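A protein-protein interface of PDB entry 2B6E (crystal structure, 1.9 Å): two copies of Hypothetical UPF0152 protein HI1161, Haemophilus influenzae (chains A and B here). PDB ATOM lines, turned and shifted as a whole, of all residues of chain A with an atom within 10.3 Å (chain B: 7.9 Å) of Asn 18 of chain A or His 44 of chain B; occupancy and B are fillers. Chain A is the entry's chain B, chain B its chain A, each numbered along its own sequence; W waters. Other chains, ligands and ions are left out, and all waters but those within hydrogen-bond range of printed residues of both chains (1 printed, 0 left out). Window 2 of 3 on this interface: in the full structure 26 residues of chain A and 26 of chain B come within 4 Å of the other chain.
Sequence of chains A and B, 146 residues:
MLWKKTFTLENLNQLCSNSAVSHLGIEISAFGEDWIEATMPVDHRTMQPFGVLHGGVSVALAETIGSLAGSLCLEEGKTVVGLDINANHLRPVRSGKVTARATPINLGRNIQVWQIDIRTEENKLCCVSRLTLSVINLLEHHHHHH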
ATOM      1  N   LEU A  12     -16.126  13.097 -19.235  1.00  0.00           N
ATOM      2  CA  LEU A  12     -16.877  13.697 -20.325  1.00  0.00           C
ATOM      3  C   LEU A  12     -18.309  13.162 -20.322  1.00  0.00           C
ATOM      4  O   LEU A  12     -19.255  13.912 -20.544  1.00  0.00           O
ATOM      5  CB  LEU A  12     -16.205  13.411 -21.671  1.00  0.00           C
ATOM      6  CG  LEU A  12     -14.857  14.095 -21.918  1.00  0.00           C
ATOM      7  CD1 LEU A  12     -14.340  13.710 -23.298  1.00  0.00           C
ATOM      8  CD2 LEU A  12     -15.009  15.610 -21.807  1.00  0.00           C
ATOM      9  N   ASN A  13     -18.476  11.867 -20.073  1.00  0.00           N
ATOM     10  CA  ASN A  13     -19.818  11.307 -20.041  1.00  0.00           C
ATOM     11  C   ASN A  13     -20.563  11.836 -18.820  1.00  0.00           C
ATOM     12  O   ASN A  13     -21.785  11.975 -18.833  1.00  0.00           O
ATOM     13  CB  ASN A  13     -19.763   9.777 -20.051  1.00  0.00           C
ATOM     14  CG  ASN A  13     -19.482   9.224 -21.441  1.00  0.00           C
ATOM     15  OD1 ASN A  13     -20.233   9.489 -22.380  1.00  0.00           O
ATOM     16  ND2 ASN A  13     -18.396   8.466 -21.581  1.00  0.00           N
ATOM     17  N   GLN A  14     -19.811  12.155 -17.772  1.00  0.00           N
ATOM     18  CA  GLN A  14     -20.390  12.706 -16.556  1.00  0.00           C
ATOM     19  C   GLN A  14     -20.911  14.097 -16.905  1.00  0.00           C
ATOM     20  O   GLN A  14     -22.030  14.459 -16.553  1.00  0.00           O
ATOM     21  CB  GLN A  14     -19.320  12.804 -15.464  1.00  0.00           C
ATOM     22  CG  GLN A  14     -19.690  12.108 -14.173  1.00  0.00           C
ATOM     23  CD  GLN A  14     -20.795  12.822 -13.420  1.00  0.00           C
ATOM     24  OE1 GLN A  14     -21.315  12.312 -12.427  1.00  0.00           O
ATOM     25  NE2 GLN A  14     -21.153  14.016 -13.884  1.00  0.00           N
ATOM     26  N   LEU A  15     -20.088  14.863 -17.616  1.00  0.00           N
ATOM     27  CA  LEU A  15     -20.440  16.216 -18.044  1.00  0.00           C
ATOM     28  C   LEU A  15     -21.715  16.226 -18.882  1.00  0.00           C
ATOM     29  O   LEU A  15     -22.517  17.158 -18.801  1.00  0.00           O
ATOM     30  CB  LEU A  15     -19.292  16.820 -18.873  1.00  0.00           C
ATOM     31  CG  LEU A  15     -19.581  18.091 -19.687  1.00  0.00           C
ATOM     32  CD1 LEU A  15     -19.865  19.255 -18.758  1.00  0.00           C
ATOM     33  CD2 LEU A  15     -18.391  18.413 -20.581  1.00  0.00           C
ATOM     34  N   CYS A  16     -21.895  15.186 -19.689  1.00  0.00           N
ATOM     35  CA  CYS A  16     -23.056  15.094 -20.568  1.00  0.00           C
ATOM     36  C   CYS A  16     -24.309  14.486 -19.932  1.00  0.00           C
ATOM     37  O   CYS A  16     -25.350  14.402 -20.582  1.00  0.00           O
ATOM     38  CB  CYS A  16     -22.685  14.300 -21.825  1.00  0.00           C
ATOM     39  SG  CYS A  16     -21.441  15.099 -22.880  1.00  0.00           S
ATOM     40  N   SER A  17     -24.218  14.069 -18.672  1.00  0.00           N
ATOM     41  CA  SER A  17     -25.370  13.462 -18.006  1.00  0.00           C
ATOM     42  C   SER A  17     -26.545  14.434 -17.874  1.00  0.00           C
ATOM     43  O   SER A  17     -26.360  15.649 -17.818  1.00  0.00           O
ATOM     44  CB  SER A  17     -24.975  12.937 -16.618  1.00  0.00           C
ATOM     45  OG  SER A  17     -24.498  13.981 -15.788  1.00  0.00           O
ATOM     46  N   ASN A  18     -27.751  13.875 -17.830  1.00  0.00           N
ATOM     47  CA  ASN A  18     -28.987  14.643 -17.709  1.00  0.00           C
ATOM     48  C   ASN A  18     -29.074  15.790 -18.712  1.00  0.00           C
ATOM     49  O   ASN A  18     -29.345  16.932 -18.343  1.00  0.00           O
ATOM     50  CB  ASN A  18     -29.140  15.192 -16.282  1.00  0.00           C
ATOM     51  CG  ASN A  18     -30.529  15.742 -16.023  1.00  0.00           C
ATOM     52  OD1 ASN A  18     -31.527  15.092 -16.334  1.00  0.00           O
ATOM     53  ND2 ASN A  18     -30.603  16.937 -15.450  1.00  0.00           N
ATOM     54  N   SER A  19     -28.841  15.476 -19.984  1.00  0.00           N
ATOM     55  CA  SER A  19     -28.898  16.472 -21.053  1.00  0.00           C
ATOM     56  C   SER A  19     -29.407  15.758 -22.295  1.00  0.00           C
ATOM     57  O   SER A  19     -29.754  14.578 -22.234  1.00  0.00           O
ATOM     58  CB  SER A  19     -27.506  17.057 -21.325  1.00  0.00           C
ATOM     59  OG  SER A  19     -26.685  16.127 -22.016  1.00  0.00           O
ATOM     60  N   ALA A  20     -29.456  16.462 -23.420  1.00  0.00           N
ATOM     61  CA  ALA A  20     -29.923  15.852 -24.660  1.00  0.00           C
ATOM     62  C   ALA A  20     -29.015  14.694 -25.055  1.00  0.00           C
ATOM     63  O   ALA A  20     -29.459  13.726 -25.679  1.00  0.00           O
ATOM     64  CB  ALA A  20     -29.960  16.897 -25.775  1.00  0.00           C
ATOM     65  N   VAL A  21     -27.742  14.790 -24.675  1.00  0.00           N
ATOM     66  CA  VAL A  21     -26.765  13.763 -25.015  1.00  0.00           C
ATOM     67  C   VAL A  21     -27.101  12.413 -24.383  1.00  0.00           C
ATOM     68  O   VAL A  21     -27.197  11.402 -25.083  1.00  0.00           O
ATOM     69  CB  VAL A  21     -25.346  14.197 -24.594  1.00  0.00           C
ATOM     70  CG1 VAL A  21     -24.322  13.172 -25.063  1.00  0.00           C
ATOM     71  CG2 VAL A  21     -25.029  15.571 -25.189  1.00  0.00           C
ATOM     72  N   SER A  22     -27.292  12.388 -23.069  1.00  0.00           N
ATOM     73  CA  SER A  22     -27.625  11.137 -22.405  1.00  0.00           C
ATOM     74  C   SER A  22     -29.031  10.692 -22.785  1.00  0.00           C
ATOM     75  O   SER A  22     -29.312   9.497 -22.857  1.00  0.00           O
ATOM     76  CB  SER A  22     -27.519  11.286 -20.885  1.00  0.00           C
ATOM     77  OG  SER A  22     -28.355  12.326 -20.409  1.00  0.00           O
ATOM     78  N   HIS A  23     -29.917  11.649 -23.037  1.00  0.00           N
ATOM     79  CA  HIS A  23     -31.289  11.318 -23.400  1.00  0.00           C
ATOM     80  C   HIS A  23     -31.350  10.531 -24.710  1.00  0.00           C
ATOM     81  O   HIS A  23     -32.277   9.747 -24.926  1.00  0.00           O
ATOM     82  CB  HIS A  23     -32.128  12.593 -23.515  1.00  0.00           C
ATOM     83  CG  HIS A  23     -33.603  12.342 -23.608  1.00  0.00           C
ATOM     84  ND1 HIS A  23     -34.317  11.720 -22.605  1.00  0.00           N
ATOM     85  CD2 HIS A  23     -34.494  12.619 -24.588  1.00  0.00           C
ATOM     86  CE1 HIS A  23     -35.585  11.623 -22.966  1.00  0.00           C
ATOM     87  NE2 HIS A  23     -35.719  12.159 -24.165  1.00  0.00           N
ATOM     88  N   LEU A  24     -30.360  10.741 -25.579  1.00  0.00           N
ATOM     89  CA  LEU A  24     -30.308  10.042 -26.863  1.00  0.00           C
ATOM     90  C   LEU A  24     -29.422   8.810 -26.776  1.00  0.00           C
ATOM     91  O   LEU A  24     -29.157   8.157 -27.784  1.00  0.00           O
ATOM     92  CB  LEU A  24     -29.798  10.987 -27.967  1.00  0.00           C
ATOM     93  CG  LEU A  24     -30.750  12.148 -28.298  1.00  0.00           C
ATOM     94  CD1 LEU A  24     -30.057  13.178 -29.205  1.00  0.00           C
ATOM     95  CD2 LEU A  24     -32.003  11.604 -28.968  1.00  0.00           C
ATOM     96  N   GLY A  25     -28.971   8.496 -25.564  1.00  0.00           N
ATOM     97  CA  GLY A  25     -28.124   7.333 -25.349  1.00  0.00           C
ATOM     98  C   GLY A  25     -26.734   7.462 -25.938  1.00  0.00           C
ATOM     99  O   GLY A  25     -26.059   6.463 -26.180  1.00  0.00           O
ATOM    100  N   ILE A  26     -26.298   8.695 -26.165  1.00  0.00           N
ATOM    101  CA  ILE A  26     -24.979   8.950 -26.730  1.00  0.00           C
ATOM    102  C   ILE A  26     -23.889   8.756 -25.684  1.00  0.00           C
ATOM    103  O   ILE A  26     -24.024   9.202 -24.544  1.00  0.00           O
ATOM    104  CB  ILE A  26     -24.889  10.389 -27.282  1.00  0.00           C
ATOM    105  CG1 ILE A  26     -25.868  10.550 -28.448  1.00  0.00           C
ATOM    106  CG2 ILE A  26     -23.462  10.702 -27.715  1.00  0.00           C
ATOM    107  CD1 ILE A  26     -26.145  12.001 -28.822  1.00  0.00           C
ATOM    108  N   LEU B  24     -38.203  13.261 -27.981  1.00  0.00           N
ATOM    109  CA  LEU B  24     -37.728  14.626 -27.791  1.00  0.00           C
ATOM    110  C   LEU B  24     -38.863  15.561 -27.372  1.00  0.00           C
ATOM    111  O   LEU B  24     -38.668  16.769 -27.254  1.00  0.00           O
ATOM    112  CB  LEU B  24     -37.102  15.144 -29.088  1.00  0.00           C
ATOM    113  CG  LEU B  24     -35.749  14.541 -29.466  1.00  0.00           C
ATOM    114  CD1 LEU B  24     -35.359  14.996 -30.871  1.00  0.00           C
ATOM    115  CD2 LEU B  24     -34.709  14.965 -28.439  1.00  0.00           C
ATOM    116  N   PRO B  41     -39.955  21.225 -26.338  1.00  0.00           N
ATOM    117  CA  PRO B  41     -39.561  21.890 -25.096  1.00  0.00           C
ATOM    118  C   PRO B  41     -38.062  22.082 -24.969  1.00  0.00           C
ATOM    119  O   PRO B  41     -37.268  21.401 -25.622  1.00  0.00           O
ATOM    120  CB  PRO B  41     -40.090  20.952 -24.021  1.00  0.00           C
ATOM    121  CG  PRO B  41     -39.857  19.588 -24.646  1.00  0.00           C
ATOM    122  CD  PRO B  41     -40.309  19.810 -26.098  1.00  0.00           C
ATOM    123  N   VAL B  42     -37.680  23.034 -24.133  1.00  0.00           N
ATOM    124  CA  VAL B  42     -36.272  23.270 -23.872  1.00  0.00           C
ATOM    125  C   VAL B  42     -36.096  22.798 -22.435  1.00  0.00           C
ATOM    126  O   VAL B  42     -36.383  23.537 -21.500  1.00  0.00           O
ATOM    127  CB  VAL B  42     -35.909  24.772 -23.976  1.00  0.00           C
ATOM    128  CG1 VAL B  42     -34.427  24.964 -23.689  1.00  0.00           C
ATOM    129  CG2 VAL B  42     -36.243  25.297 -25.367  1.00  0.00           C
ATOM    130  N   ASP B  43     -35.686  21.545 -22.266  1.00  0.00           N
ATOM    131  CA  ASP B  43     -35.466  20.972 -20.941  1.00  0.00           C
ATOM    132  C   ASP B  43     -34.306  19.984 -21.010  1.00  0.00           C
ATOM    133  O   ASP B  43     -33.590  19.950 -22.010  1.00  0.00           O
ATOM    134  CB  ASP B  43     -36.742  20.292 -20.401  1.00  0.00           C
ATOM    135  CG  ASP B  43     -37.240  19.156 -21.284  1.00  0.00           C
ATOM    136  OD1 ASP B  43     -36.461  18.627 -22.095  1.00  0.00           O
ATOM    137  OD2 ASP B  43     -38.425  18.778 -21.148  1.00  0.00           O
ATOM    138  N   HIS B  44     -34.113  19.177 -19.969  1.00  0.00           N
ATOM    139  CA  HIS B  44     -32.989  18.245 -19.966  1.00  0.00           C
ATOM    140  C   HIS B  44     -32.965  17.252 -21.121  1.00  0.00           C
ATOM    141  O   HIS B  44     -31.921  16.664 -21.412  1.00  0.00           O
ATOM    142  CB  HIS B  44     -32.905  17.486 -18.632  1.00  0.00           C
ATOM    143  CG  HIS B  44     -33.973  16.456 -18.443  1.00  0.00           C
ATOM    144  ND1 HIS B  44     -35.230  16.762 -17.966  1.00  0.00           N
ATOM    145  CD2 HIS B  44     -33.973  15.123 -18.672  1.00  0.00           C
ATOM    146  CE1 HIS B  44     -35.957  15.661 -17.911  1.00  0.00           C
ATOM    147  NE2 HIS B  44     -35.220  14.650 -18.334  1.00  0.00           N
ATOM    148  N   ARG B  45     -34.105  17.055 -21.776  1.00  0.00           N
ATOM    149  CA  ARG B  45     -34.176  16.130 -22.909  1.00  0.00           C
ATOM    150  C   ARG B  45     -33.597  16.772 -24.166  1.00  0.00           C
ATOM    151  O   ARG B  45     -33.139  16.075 -25.079  1.00  0.00           O
ATOM    152  CB  ARG B  45     -35.632  15.756 -23.210  1.00  0.00           C
ATOM    153  CG  ARG B  45     -36.331  14.919 -22.161  1.00  0.00           C
ATOM    154  CD  ARG B  45     -37.802  14.736 -22.511  1.00  0.00           C
ATOM    155  NE  ARG B  45     -38.554  15.975 -22.358  1.00  0.00           N
ATOM    156  CZ  ARG B  45     -39.848  16.110 -22.633  1.00  0.00           C
ATOM    157  NH1 ARG B  45     -40.545  15.079 -23.090  1.00  0.00           N
ATOM    158  NH2 ARG B  45     -40.453  17.272 -22.424  1.00  0.00           N
ATOM    159  N   THR B  46     -33.622  18.099 -24.210  1.00  0.00           N
ATOM    160  CA  THR B  46     -33.176  18.818 -25.398  1.00  0.00           C
ATOM    161  C   THR B  46     -32.092  19.883 -25.220  1.00  0.00           C
ATOM    162  O   THR B  46     -31.753  20.581 -26.185  1.00  0.00           O
ATOM    163  CB  THR B  46     -34.376  19.490 -26.056  1.00  0.00           C
ATOM    164  OG1 THR B  46     -34.874  20.515 -25.185  1.00  0.00           O
ATOM    165  CG2 THR B  46     -35.492  18.471 -26.283  1.00  0.00           C
ATOM    166  N   MET B  47     -31.554  20.012 -24.011  1.00  0.00           N
ATOM    167  CA  MET B  47     -30.521  21.012 -23.740  1.00  0.00           C
ATOM    168  C   MET B  47     -29.113  20.434 -23.703  1.00  0.00           C
ATOM    169  O   MET B  47     -28.919  19.240 -23.456  1.00  0.00           O
ATOM    170  CB  MET B  47     -30.754  21.686 -22.388  1.00  0.00           C
ATOM    171  CG  MET B  47     -32.031  22.480 -22.229  1.00  0.00           C
ATOM    172  SD  MET B  47     -32.169  23.092 -20.378  1.00  0.00           S
ATOM    173  CE  MET B  47     -31.633  21.484 -19.474  1.00  0.00           C
ATOM    174  N   GLN B  48     -28.128  21.293 -23.940  1.00  0.00           N
ATOM    175  CA  GLN B  48     -26.740  20.872 -23.858  1.00  0.00           C
ATOM    176  C   GLN B  48     -26.446  20.852 -22.360  1.00  0.00           C
ATOM    177  O   GLN B  48     -27.212  21.402 -21.565  1.00  0.00           O
ATOM    178  CB  GLN B  48     -25.831  21.868 -24.582  1.00  0.00           C
ATOM    179  CG  GLN B  48     -25.892  21.743 -26.094  1.00  0.00           C
ATOM    180  CD  GLN B  48     -25.036  22.768 -26.808  1.00  0.00           C
ATOM    181  OE1 GLN B  48     -25.323  23.966 -26.774  1.00  0.00           O
ATOM    182  NE2 GLN B  48     -23.976  22.301 -27.462  1.00  0.00           N
ATOM    183  N   PRO B  49     -25.343  20.216 -21.949  1.00  0.00           N
ATOM    184  CA  PRO B  49     -25.033  20.171 -20.519  1.00  0.00           C
ATOM    185  C   PRO B  49     -24.929  21.516 -19.791  1.00  0.00           C
ATOM    186  O   PRO B  49     -24.951  21.551 -18.560  1.00  0.00           O
ATOM    187  CB  PRO B  49     -23.735  19.359 -20.468  1.00  0.00           C
ATOM    188  CG  PRO B  49     -23.115  19.600 -21.801  1.00  0.00           C
ATOM    189  CD  PRO B  49     -24.300  19.539 -22.737  1.00  0.00           C
ATOM    190  N   PHE B  50     -24.840  22.620 -20.525  1.00  0.00           N
ATOM    191  CA  PHE B  50     -24.736  23.918 -19.862  1.00  0.00           C
ATOM    192  C   PHE B  50     -26.004  24.764 -19.764  1.00  0.00           C
ATOM    193  O   PHE B  50     -25.927  25.975 -19.560  1.00  0.00           O
ATOM    194  CB  PHE B  50     -23.618  24.759 -20.481  1.00  0.00           C
ATOM    195  CG  PHE B  50     -23.458  24.572 -21.954  1.00  0.00           C
ATOM    196  CD1 PHE B  50     -22.750  23.480 -22.454  1.00  0.00           C
ATOM    197  CD2 PHE B  50     -24.002  25.487 -22.851  1.00  0.00           C
ATOM    198  CE1 PHE B  50     -22.581  23.305 -23.824  1.00  0.00           C
ATOM    199  CE2 PHE B  50     -23.842  25.322 -24.226  1.00  0.00           C
ATOM    200  CZ  PHE B  50     -23.129  24.228 -24.712  1.00  0.00           C
ATOM    201  N   GLY B  51     -27.168  24.144 -19.928  1.00  0.00           N
ATOM    202  CA  GLY B  51     -28.405  24.892 -19.770  1.00  0.00           C
ATOM    203  C   GLY B  51     -29.101  25.581 -20.928  1.00  0.00           C
ATOM    204  O   GLY B  51     -30.083  26.294 -20.709  1.00  0.00           O
ATOM    205  N   HIS B  54     -29.903  22.511 -27.176  1.00  0.00           N
ATOM    206  CA  HIS B  54     -28.849  21.847 -27.940  1.00  0.00           C
ATOM    207  C   HIS B  54     -29.058  22.101 -29.439  1.00  0.00           C
ATOM    208  O   HIS B  54     -30.079  21.705 -30.010  1.00  0.00           O
ATOM    209  CB  HIS B  54     -28.889  20.345 -27.622  1.00  0.00           C
ATOM    210  CG  HIS B  54     -27.745  19.561 -28.184  1.00  0.00           C
ATOM    211  ND1 HIS B  54     -27.505  19.456 -29.537  1.00  0.00           N
ATOM    212  CD2 HIS B  54     -26.807  18.796 -27.576  1.00  0.00           C
ATOM    213  CE1 HIS B  54     -26.470  18.659 -29.738  1.00  0.00           C
ATOM    214  NE2 HIS B  54     -26.029  18.244 -28.564  1.00  0.00           N
HETATM  215  O   HOH W   1     -31.788  13.958 -20.153  1.00  0.00           O
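The backbone carbonyl oxygen of His 44 of chain B sits at hydrogen-bond distance from the backbone NH of Ala 20 of chain A, 3.2 Å away.
O of His 44 of chain B lies close to O of Ser 19 of chain A (3.1 Å).
The backbone carbonyl oxygen of Met 47 of chain B lies within hydrogen-bond range of the backbone NH of Ala 20 of chain A.
N of Asn 18 of chain A lies within hydrogen-bond range of OG of Ser 22 of chain A, at 3.1 Å.
N of His 54 of chain B lies within hydrogen-bond range of O of Thr 46 of chain B, 2.9 Å away.
The side-chain carboxylate of Asp 43 of chain B is in salt-bridge range of the guanidinium group of Arg 45 of chain B, 2.8 Å away.
OG of Ser 19 of chain A lies close to N of Val 21 of chain A, at 3.2 Å.
The side-chain hydroxyl (OG) of Ser 19 of chain A is in hydrogen-bond range of the backbone carbonyl oxygen (O) of Cys 16 of chain A, 2.6 Å away.
The side-chain hydroxyl (OG1) of Thr 46 of chain B is in hydrogen-bond range of the backbone NH (N) of Asp 43 of chain B, 3.2 Å away.
Among the printed residues, pairs that only touch across the chains: Leu 15 of chain A with Pro 49 of chain B (3.0 Å), Asn 18 of chain A with His 44 of chain B (3.4 Å), Ser 19 of chain A with Met 47 of chain B (3.4 Å), Ser 19 of chain A with Pro 49 of chain B (3.9 Å), Ala 20 of chain A with Arg 45 of chain B (3.3 Å), Ala 20 of chain A with Thr 46 of chain B (3.7 Å) and His 23 of chain A with Arg 45 of chain B (3.5 Å).
No residue of chain B comes within 4 Å of Ser 17 of chain A.
Of chain B, only His 44 comes within 4 Å of Asn 18 of chain A.
Of the printed residues of chain B, Ser 19 of chain A touches His 44, Met 47 and Pro 49.
Of the printed residues of chain B, Ala 20 of chain A touches His 44 (3.2 Å), Arg 45 (3.3 Å), Thr 46 (3.7 Å) and Met 47 (2.8 Å).
Ser 22 of chain A touches none of the printed residues of chain B.
Of the printed residues of chain B, His 23 of chain A touches Arg 45 (3.5 Å).
Leu 24 of chain A touches none of the printed residues of chain B.
No residue of chain A comes within 4 Å of Asp 43 of chain B.
Of chain A, only Asn 18, Ser 19 and Ala 20 come within 4 Å of His 44 of chain B.
Of the printed residues of chain A, Arg 45 of chain B touches Ala 20 (3.3 Å) and His 23 (3.5 Å).
Of chain A, only Ser 19 and Ala 20 come within 4 Å of Met 47 of chain B.
Of the printed residues of chain A, Pro 49 of chain B touches Leu 15 and Ser 19.
Of the 13 printed residues of chain B, 5 touch a printed residue of chain A.
Hydrophobic or aromatic side chains of chain B that line the printed part of chain A: His 44 and Pro 49.
Along chain B the printed residues that touch a printed residue of chain A span positions 44 to 49.
Of the 15 printed residues of chain A, 5 touch a printed residue of chain B.
Hydrophobic or aromatic side chains of chain A that line the printed part of chain B: Ala 20 and His 23.
Among the printed residues, no Asp or Glu carboxylate lies within 4 Å of a Lys or Arg side-chain nitrogen of the other chain.
Position printed for both chains: 24.
Water W1 bridges O of Ser 19 of chain A and O of His 44 of chain B.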
